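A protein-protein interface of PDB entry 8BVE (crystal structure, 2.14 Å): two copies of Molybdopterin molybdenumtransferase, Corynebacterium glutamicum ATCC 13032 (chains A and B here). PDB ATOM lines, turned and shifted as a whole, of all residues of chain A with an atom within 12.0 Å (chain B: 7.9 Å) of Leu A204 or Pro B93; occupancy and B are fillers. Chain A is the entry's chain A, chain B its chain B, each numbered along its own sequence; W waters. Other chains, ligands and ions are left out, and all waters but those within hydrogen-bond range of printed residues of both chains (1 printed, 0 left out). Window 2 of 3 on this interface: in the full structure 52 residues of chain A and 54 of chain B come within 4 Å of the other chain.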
ATOM      1  N   GLY A 192     -20.467   7.125  16.179  1.00  0.00           N
ATOM      2  CA  GLY A 192     -20.455   8.465  15.627  1.00  0.00           C
ATOM      3  C   GLY A 192     -19.535   9.399  16.381  1.00  0.00           C
ATOM      4  O   GLY A 192     -19.597   9.489  17.612  1.00  0.00           O
ATOM      5  N   ALA A 193     -18.674  10.102  15.644  1.00  0.00           N
ATOM      6  CA  ALA A 193     -17.733  11.023  16.266  1.00  0.00           C
ATOM      7  C   ALA A 193     -18.429  12.141  17.028  1.00  0.00           C
ATOM      8  O   ALA A 193     -17.827  12.722  17.935  1.00  0.00           O
ATOM      9  CB  ALA A 193     -16.809  11.623  15.199  1.00  0.00           C
ATOM     10  N   GLU A 194     -19.683  12.445  16.695  1.00  0.00           N
ATOM     11  CA  GLU A 194     -20.402  13.516  17.370  1.00  0.00           C
ATOM     12  C   GLU A 194     -20.983  13.100  18.719  1.00  0.00           C
ATOM     13  O   GLU A 194     -21.373  13.976  19.498  1.00  0.00           O
ATOM     14  CB  GLU A 194     -21.520  14.043  16.459  1.00  0.00           C
ATOM     15  CG  GLU A 194     -22.776  13.171  16.415  1.00  0.00           C
ATOM     16  CD  GLU A 194     -22.653  11.992  15.455  1.00  0.00           C
ATOM     17  OE1 GLU A 194     -21.552  11.770  14.908  1.00  0.00           O
ATOM     18  OE2 GLU A 194     -23.661  11.284  15.253  1.00  0.00           O
ATOM     19  N   LEU A 195     -21.024  11.806  19.030  1.00  0.00           N
ATOM     20  CA  LEU A 195     -21.792  11.333  20.174  1.00  0.00           C
ATOM     21  C   LEU A 195     -21.030  11.519  21.480  1.00  0.00           C
ATOM     22  O   LEU A 195     -19.822  11.279  21.552  1.00  0.00           O
ATOM     23  CB  LEU A 195     -22.158   9.859  19.995  1.00  0.00           C
ATOM     24  CG  LEU A 195     -23.038   9.519  18.786  1.00  0.00           C
ATOM     25  CD1 LEU A 195     -23.259   8.016  18.678  1.00  0.00           C
ATOM     26  CD2 LEU A 195     -24.363  10.260  18.852  1.00  0.00           C
ATOM     27  N   VAL A 196     -21.749  11.966  22.512  1.00  0.00           N
ATOM     28  CA  VAL A 196     -21.246  11.991  23.878  1.00  0.00           C
ATOM     29  C   VAL A 196     -22.308  11.384  24.781  1.00  0.00           C
ATOM     30  O   VAL A 196     -23.506  11.438  24.481  1.00  0.00           O
ATOM     31  CB  VAL A 196     -20.882  13.416  24.361  1.00  0.00           C
ATOM     32  CG1 VAL A 196     -19.689  13.949  23.591  1.00  0.00           C
ATOM     33  CG2 VAL A 196     -22.085  14.356  24.239  1.00  0.00           C
ATOM     34  N   ASP A 197     -21.864  10.802  25.894  1.00  0.00           N
ATOM     35  CA  ASP A 197     -22.808  10.247  26.850  1.00  0.00           C
ATOM     36  C   ASP A 197     -23.538  11.374  27.580  1.00  0.00           C
ATOM     37  O   ASP A 197     -23.137  12.540  27.547  1.00  0.00           O
ATOM     38  CB  ASP A 197     -22.098   9.332  27.845  1.00  0.00           C
ATOM     39  CG  ASP A 197     -23.032   8.293  28.456  1.00  0.00           C
ATOM     40  OD1 ASP A 197     -24.192   8.172  27.998  1.00  0.00           O
ATOM     41  OD2 ASP A 197     -22.605   7.597  29.397  1.00  0.00           O
ATOM     42  N   ARG A 200     -22.180  14.014  30.285  1.00  0.00           N
ATOM     43  CA  ARG A 200     -21.189  14.980  29.846  1.00  0.00           C
ATOM     44  C   ARG A 200     -21.880  16.263  29.405  1.00  0.00           C
ATOM     45  O   ARG A 200     -23.080  16.290  29.124  1.00  0.00           O
ATOM     46  CB  ARG A 200     -20.348  14.416  28.693  1.00  0.00           C
ATOM     47  CG  ARG A 200     -19.089  13.667  29.116  1.00  0.00           C
ATOM     48  CD  ARG A 200     -17.880  14.113  28.285  1.00  0.00           C
ATOM     49  NE  ARG A 200     -17.496  13.134  27.273  1.00  0.00           N
ATOM     50  CZ  ARG A 200     -16.781  13.414  26.191  1.00  0.00           C
ATOM     51  NH1 ARG A 200     -16.352  14.640  25.945  1.00  0.00           N
ATOM     52  NH2 ARG A 200     -16.493  12.440  25.330  1.00  0.00           N
ATOM     53  N   GLN A 201     -21.093  17.330  29.337  1.00  0.00           N
ATOM     54  CA  GLN A 201     -21.560  18.602  28.815  1.00  0.00           C
ATOM     55  C   GLN A 201     -21.129  18.669  27.362  1.00  0.00           C
ATOM     56  O   GLN A 201     -19.922  18.743  27.090  1.00  0.00           O
ATOM     57  CB  GLN A 201     -20.972  19.770  29.606  1.00  0.00           C
ATOM     58  CG  GLN A 201     -21.699  21.093  29.407  1.00  0.00           C
ATOM     59  CD  GLN A 201     -23.179  21.008  29.734  1.00  0.00           C
ATOM     60  OE1 GLN A 201     -24.031  21.353  28.911  1.00  0.00           O
ATOM     61  NE2 GLN A 201     -23.495  20.540  30.938  1.00  0.00           N
ATOM     62  N   PRO A 202     -22.054  18.610  26.405  1.00  0.00           N
ATOM     63  CA  PRO A 202     -21.652  18.562  24.993  1.00  0.00           C
ATOM     64  C   PRO A 202     -20.892  19.816  24.594  1.00  0.00           C
ATOM     65  O   PRO A 202     -21.316  20.937  24.878  1.00  0.00           O
ATOM     66  CB  PRO A 202     -22.986  18.450  24.244  1.00  0.00           C
ATOM     67  CG  PRO A 202     -23.989  18.021  25.276  1.00  0.00           C
ATOM     68  CD  PRO A 202     -23.515  18.606  26.568  1.00  0.00           C
ATOM     69  N   GLY A 203     -19.754  19.612  23.939  1.00  0.00           N
ATOM     70  CA  GLY A 203     -18.984  20.692  23.370  1.00  0.00           C
ATOM     71  C   GLY A 203     -19.443  20.994  21.962  1.00  0.00           C
ATOM     72  O   GLY A 203     -20.530  20.594  21.533  1.00  0.00           O
ATOM     73  N   LEU A 204     -18.591  21.707  21.231  1.00  0.00           N
ATOM     74  CA  LEU A 204     -18.896  22.049  19.848  1.00  0.00           C
ATOM     75  C   LEU A 204     -19.054  20.793  18.998  1.00  0.00           C
ATOM     76  O   LEU A 204     -18.205  19.896  19.024  1.00  0.00           O
ATOM     77  CB  LEU A 204     -17.797  22.946  19.275  1.00  0.00           C
ATOM     78  CG  LEU A 204     -18.131  24.434  19.161  1.00  0.00           C
ATOM     79  CD1 LEU A 204     -18.131  25.106  20.528  1.00  0.00           C
ATOM     80  CD2 LEU A 204     -17.151  25.129  18.227  1.00  0.00           C
ATOM     81  N   GLY A 205     -20.165  20.718  18.270  1.00  0.00           N
ATOM     82  CA  GLY A 205     -20.402  19.607  17.375  1.00  0.00           C
ATOM     83  C   GLY A 205     -20.874  18.329  18.027  1.00  0.00           C
ATOM     84  O   GLY A 205     -21.083  17.339  17.320  1.00  0.00           O
ATOM     85  N   GLN A 206     -21.089  18.320  19.337  1.00  0.00           N
ATOM     86  CA  GLN A 206     -21.378  17.081  20.041  1.00  0.00           C
ATOM     87  C   GLN A 206     -22.868  16.958  20.328  1.00  0.00           C
ATOM     88  O   GLN A 206     -23.555  17.943  20.611  1.00  0.00           O
ATOM     89  CB  GLN A 206     -20.574  16.994  21.341  1.00  0.00           C
ATOM     90  CG  GLN A 206     -19.069  16.868  21.104  1.00  0.00           C
ATOM     91  CD  GLN A 206     -18.268  16.801  22.388  1.00  0.00           C
ATOM     92  OE1 GLN A 206     -18.545  17.524  23.345  1.00  0.00           O
ATOM     93  NE2 GLN A 206     -17.266  15.928  22.415  1.00  0.00           N
ATOM     94  N   VAL A 207     -23.347  15.718  20.268  1.00  0.00           N
ATOM     95  CA  VAL A 207     -24.761  15.373  20.338  1.00  0.00           C
ATOM     96  C   VAL A 207     -24.917  14.258  21.364  1.00  0.00           C
ATOM     97  O   VAL A 207     -24.099  13.334  21.409  1.00  0.00           O
ATOM     98  CB  VAL A 207     -25.264  14.914  18.947  1.00  0.00           C
ATOM     99  CG1 VAL A 207     -26.708  14.445  18.987  1.00  0.00           C
ATOM    100  CG2 VAL A 207     -25.058  16.016  17.900  1.00  0.00           C
ATOM    101  N   TYR A 208     -25.960  14.343  22.190  1.00  0.00           N
ATOM    102  CA  TYR A 208     -26.223  13.290  23.163  1.00  0.00           C
ATOM    103  C   TYR A 208     -26.537  11.973  22.466  1.00  0.00           C
ATOM    104  O   TYR A 208     -27.255  11.939  21.462  1.00  0.00           O
ATOM    105  CB  TYR A 208     -27.388  13.680  24.069  1.00  0.00           C
ATOM    106  CG  TYR A 208     -27.041  14.690  25.138  1.00  0.00           C
ATOM    107  CD1 TYR A 208     -25.985  14.470  26.011  1.00  0.00           C
ATOM    108  CD2 TYR A 208     -27.782  15.857  25.283  1.00  0.00           C
ATOM    109  CE1 TYR A 208     -25.667  15.386  26.993  1.00  0.00           C
ATOM    110  CE2 TYR A 208     -27.473  16.781  26.265  1.00  0.00           C
ATOM    111  CZ  TYR A 208     -26.417  16.534  27.122  1.00  0.00           C
ATOM    112  OH  TYR A 208     -26.101  17.440  28.103  1.00  0.00           O
ATOM    113  N   PHE B  46     -27.404  22.854  18.603  1.00  0.00           N
ATOM    114  CA  PHE B  46     -26.732  23.811  17.739  1.00  0.00           C
ATOM    115  C   PHE B  46     -27.385  23.732  16.367  1.00  0.00           C
ATOM    116  O   PHE B  46     -27.987  22.716  16.014  1.00  0.00           O
ATOM    117  CB  PHE B  46     -25.219  23.543  17.650  1.00  0.00           C
ATOM    118  CG  PHE B  46     -24.870  22.123  17.295  1.00  0.00           C
ATOM    119  CD1 PHE B  46     -24.801  21.146  18.276  1.00  0.00           C
ATOM    120  CD2 PHE B  46     -24.613  21.766  15.981  1.00  0.00           C
ATOM    121  CE1 PHE B  46     -24.486  19.839  17.953  1.00  0.00           C
ATOM    122  CE2 PHE B  46     -24.295  20.456  15.653  1.00  0.00           C
ATOM    123  CZ  PHE B  46     -24.229  19.493  16.638  1.00  0.00           C
ATOM    124  N   VAL B  86     -17.239  21.015   6.713  1.00  0.00           N
ATOM    125  CA  VAL B  86     -17.652  20.617   8.052  1.00  0.00           C
ATOM    126  C   VAL B  86     -18.420  19.305   7.962  1.00  0.00           C
ATOM    127  O   VAL B  86     -19.413  19.207   7.228  1.00  0.00           O
ATOM    128  CB  VAL B  86     -18.515  21.697   8.721  1.00  0.00           C
ATOM    129  CG1 VAL B  86     -18.810  21.314  10.160  1.00  0.00           C
ATOM    130  CG2 VAL B  86     -17.825  23.044   8.655  1.00  0.00           C
ATOM    131  N   ALA B  88     -20.228  16.025  10.386  1.00  0.00           N
ATOM    132  CA  ALA B  88     -20.837  15.811  11.692  1.00  0.00           C
ATOM    133  C   ALA B  88     -19.757  15.506  12.724  1.00  0.00           C
ATOM    134  O   ALA B  88     -18.804  14.773  12.451  1.00  0.00           O
ATOM    135  CB  ALA B  88     -21.849  14.665  11.625  1.00  0.00           C
ATOM    136  N   GLY B  89     -19.894  16.100  13.909  1.00  0.00           N
ATOM    137  CA  GLY B  89     -18.909  15.923  14.954  1.00  0.00           C
ATOM    138  C   GLY B  89     -17.759  16.908  14.937  1.00  0.00           C
ATOM    139  O   GLY B  89     -16.897  16.840  15.825  1.00  0.00           O
ATOM    140  N   SER B  90     -17.729  17.834  13.975  1.00  0.00           N
ATOM    141  CA  SER B  90     -16.651  18.812  13.897  1.00  0.00           C
ATOM    142  C   SER B  90     -16.579  19.652  15.165  1.00  0.00           C
ATOM    143  O   SER B  90     -17.588  20.180  15.639  1.00  0.00           O
ATOM    144  CB  SER B  90     -16.845  19.722  12.684  1.00  0.00           C
ATOM    145  OG  SER B  90     -16.043  20.887  12.799  1.00  0.00           O
ATOM    146  N   GLN B  91     -15.373  19.764  15.715  1.00  0.00           N
ATOM    147  CA  GLN B  91     -15.122  20.499  16.945  1.00  0.00           C
ATOM    148  C   GLN B  91     -14.440  21.832  16.688  1.00  0.00           C
ATOM    149  O   GLN B  91     -14.031  22.503  17.640  1.00  0.00           O
ATOM    150  CB  GLN B  91     -14.275  19.658  17.903  1.00  0.00           C
ATOM    151  CG  GLN B  91     -14.892  18.324  18.268  1.00  0.00           C
ATOM    152  CD  GLN B  91     -14.721  18.002  19.736  1.00  0.00           C
ATOM    153  OE1 GLN B  91     -15.513  18.441  20.575  1.00  0.00           O
ATOM    154  NE2 GLN B  91     -13.677  17.245  20.061  1.00  0.00           N
ATOM    155  N   GLN B  92     -14.311  22.234  15.427  1.00  0.00           N
ATOM    156  CA  GLN B  92     -13.621  23.503  15.290  1.00  0.00           C
ATOM    157  C   GLN B  92     -14.611  24.619  14.997  1.00  0.00           C
ATOM    158  O   GLN B  92     -15.546  24.433  14.208  1.00  0.00           O
ATOM    159  CB  GLN B  92     -12.589  23.437  14.163  1.00  0.00           C
ATOM    160  N   PRO B  93     -14.451  25.775  15.638  1.00  0.00           N
ATOM    161  CA  PRO B  93     -15.330  26.901  15.322  1.00  0.00           C
ATOM    162  C   PRO B  93     -15.049  27.413  13.919  1.00  0.00           C
ATOM    163  O   PRO B  93     -13.903  27.433  13.464  1.00  0.00           O
ATOM    164  CB  PRO B  93     -14.976  27.952  16.384  1.00  0.00           C
ATOM    165  CG  PRO B  93     -13.848  27.372  17.209  1.00  0.00           C
ATOM    166  CD  PRO B  93     -13.320  26.172  16.492  1.00  0.00           C
ATOM    167  N   LEU B  94     -16.111  27.819  13.233  1.00  0.00           N
ATOM    168  CA  LEU B  94     -16.007  28.394  11.901  1.00  0.00           C
ATOM    169  C   LEU B  94     -16.999  29.538  11.795  1.00  0.00           C
ATOM    170  O   LEU B  94     -18.178  29.368  12.122  1.00  0.00           O
ATOM    171  CB  LEU B  94     -16.294  27.359  10.807  1.00  0.00           C
ATOM    172  CG  LEU B  94     -15.163  26.924   9.879  1.00  0.00           C
ATOM    173  CD1 LEU B  94     -15.707  25.951   8.852  1.00  0.00           C
ATOM    174  CD2 LEU B  94     -14.529  28.128   9.194  1.00  0.00           C
ATOM    175  N   ARG B  95     -16.520  30.691  11.344  1.00  0.00           N
ATOM    176  CA  ARG B  95     -17.336  31.883  11.158  1.00  0.00           C
ATOM    177  C   ARG B  95     -17.394  32.194   9.671  1.00  0.00           C
ATOM    178  O   ARG B  95     -16.354  32.252   9.009  1.00  0.00           O
ATOM    179  CB  ARG B  95     -16.774  33.074  11.935  1.00  0.00           C
ATOM    180  CG  ARG B  95     -16.319  32.722  13.342  1.00  0.00           C
ATOM    181  CD  ARG B  95     -15.923  33.964  14.125  1.00  0.00           C
ATOM    182  NE  ARG B  95     -17.077  34.677  14.661  1.00  0.00           N
ATOM    183  CZ  ARG B  95     -17.414  35.915  14.326  1.00  0.00           C
ATOM    184  NH1 ARG B  95     -16.701  36.616  13.459  1.00  0.00           N
ATOM    185  NH2 ARG B  95     -18.486  36.469  14.887  1.00  0.00           N
ATOM    186  N   LEU B  96     -18.598  32.372   9.144  1.00  0.00           N
ATOM    187  CA  LEU B  96     -18.776  32.691   7.735  1.00  0.00           C
ATOM    188  C   LEU B  96     -18.737  34.203   7.536  1.00  0.00           C
ATOM    189  O   LEU B  96     -19.516  34.938   8.156  1.00  0.00           O
ATOM    190  CB  LEU B  96     -20.097  32.118   7.225  1.00  0.00           C
ATOM    191  CG  LEU B  96     -20.259  32.055   5.706  1.00  0.00           C
ATOM    192  CD1 LEU B  96     -19.519  30.846   5.137  1.00  0.00           C
ATOM    193  CD2 LEU B  96     -21.733  32.024   5.327  1.00  0.00           C
ATOM    194  N   PRO B 109     -22.406  20.884  12.191  1.00  0.00           N
ATOM    195  CA  PRO B 109     -22.682  22.173  12.833  1.00  0.00           C
ATOM    196  C   PRO B 109     -22.542  23.305  11.825  1.00  0.00           C
ATOM    197  O   PRO B 109     -21.526  23.421  11.133  1.00  0.00           O
ATOM    198  CB  PRO B 109     -21.624  22.261  13.938  1.00  0.00           C
ATOM    199  CG  PRO B 109     -20.532  21.338  13.504  1.00  0.00           C
ATOM    200  CD  PRO B 109     -21.185  20.244  12.712  1.00  0.00           C
ATOM    201  N   LEU B 110     -23.578  24.128  11.741  1.00  0.00           N
ATOM    202  CA  LEU B 110     -23.560  25.262  10.834  1.00  0.00           C
ATOM    203  C   LEU B 110     -22.498  26.266  11.275  1.00  0.00           C
ATOM    204  O   LEU B 110     -22.362  26.540  12.472  1.00  0.00           O
ATOM    205  CB  LEU B 110     -24.936  25.929  10.795  1.00  0.00           C
ATOM    206  CG  LEU B 110     -25.340  26.704   9.539  1.00  0.00           C
ATOM    207  CD1 LEU B 110     -25.748  25.753   8.429  1.00  0.00           C
ATOM    208  CD2 LEU B 110     -26.472  27.669   9.854  1.00  0.00           C
ATOM    209  N   PRO B 111     -21.707  26.799  10.346  1.00  0.00           N
ATOM    210  CA  PRO B 111     -20.798  27.898  10.697  1.00  0.00           C
ATOM    211  C   PRO B 111     -21.560  29.072  11.292  1.00  0.00           C
ATOM    212  O   PRO B 111     -22.701  29.353  10.912  1.00  0.00           O
ATOM    213  CB  PRO B 111     -20.153  28.283   9.358  1.00  0.00           C
ATOM    214  CG  PRO B 111     -20.432  27.168   8.417  1.00  0.00           C
ATOM    215  CD  PRO B 111     -21.537  26.318   8.964  1.00  0.00           C
ATOM    216  N   MET B 112     -20.936  29.735  12.264  1.00  0.00           N
ATOM    217  CA  MET B 112     -21.500  30.973  12.787  1.00  0.00           C
ATOM    218  C   MET B 112     -21.660  31.988  11.664  1.00  0.00           C
ATOM    219  O   MET B 112     -20.831  32.059  10.752  1.00  0.00           O
ATOM    220  CB  MET B 112     -20.615  31.563  13.888  1.00  0.00           C
ATOM    221  CG  MET B 112     -20.193  30.572  14.956  1.00  0.00           C
ATOM    222  SD  MET B 112     -21.550  30.154  16.074  1.00  0.00           S
ATOM    223  CE  MET B 112     -21.902  28.473  15.554  1.00  0.00           C
HETATM  224  O   HOH W   1     -22.010  17.370  14.818  1.00  0.00           O
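Among the printed residues, pairs that only touch across the chains: Gly A205 with Ser B90, Gln A206 with Phe B46, Gly A205 with Gly B89, Glu A194 with Gly B89, Gln A206 with Gln B91, Val A207 with Phe B46, Leu A204 with Pro B93 and Gly A205 with Phe B46.
The backbone carbonyl oxygen (O) of Leu A204 lies close to the side-chain amide oxygen (OE1) of Gln B91 (3.4 Å). The backbone carbonyl oxygen of Leu A204 sits close to the backbone carbonyl oxygen of Ser B90 (3.5 Å).
The backbone NH (N) of Val A207 lies within hydrogen-bond range of the backbone carbonyl oxygen (O) of Glu A194. N of Val A196 lies within hydrogen-bond range of O of Val A207, at 2.9 Å. N of Gly A203 sits at hydrogen-bond distance from OE1 of Gln A206 (2.5 Å). The side-chain hydroxyl (OG) of Ser B90 lies within hydrogen-bond range of the backbone NH (N) of Gln B92 (3.4 Å).
Of the 15 printed residues of chain A, 5 touch a printed residue of chain B. Printed residues of chain A that touch a printed residue of chain B: Glu A194, Leu A204, Gly A205, Gln A206 and Val A207. Hydrophobic or aromatic side chains of chain A that line the printed part of chain B: Leu A204 and Val A207. Along chain A the printed residues that touch a printed residue of chain B span positions 194 to 207. Of the 15 printed residues of chain B, 5 touch a printed residue of chain A. Among the printed residues, no Asp or Glu carboxylate lies within 4 Å of a Lys or Arg side-chain nitrogen of the other chain.
Water W1 bridges N of Gly B89 (2.6 Å) and O of Gly A205 (2.7 Å).
Of the printed residues of chain B, Glu A194 touches Gly B89 (3.6 Å). Val A196 touches none of the printed residues of chain B. Gly A203 touches none of the printed residues of chain B. Of the printed residues of chain B, Gly A205 touches Phe B46, Gly B89 and Ser B90. Of the printed residues of chain B, Gln A206 touches Phe B46 (3.4 Å) and Gln B91 (3.6 Å). Of the printed residues of chain B, Val A207 touches Phe B46 (3.8 Å). Of the printed residues of chain A, Phe B46 touches Gly A205 (3.8 Å), Gln A206 (3.4 Å) and Val A207 (3.8 Å). Gly B89 touches just these residues of chain A: Glu A194 (3.6 Å) and Gly A205 (3.5 Å). Ser B90 touches two residues of chain A. Of chain A, only Leu A204 and Gln A206 come within 4 Å of Gln B91. Pro B93 touches just one residue of chain A: Leu A204. The nearest residue of chain B that does not touch Leu A204 is Gln B92 (4.1 Å).
No position is printed for both chains. Of the 10 pairs that touch across the chains among the printed residues, none has its exchanged pair printed and touching as well.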
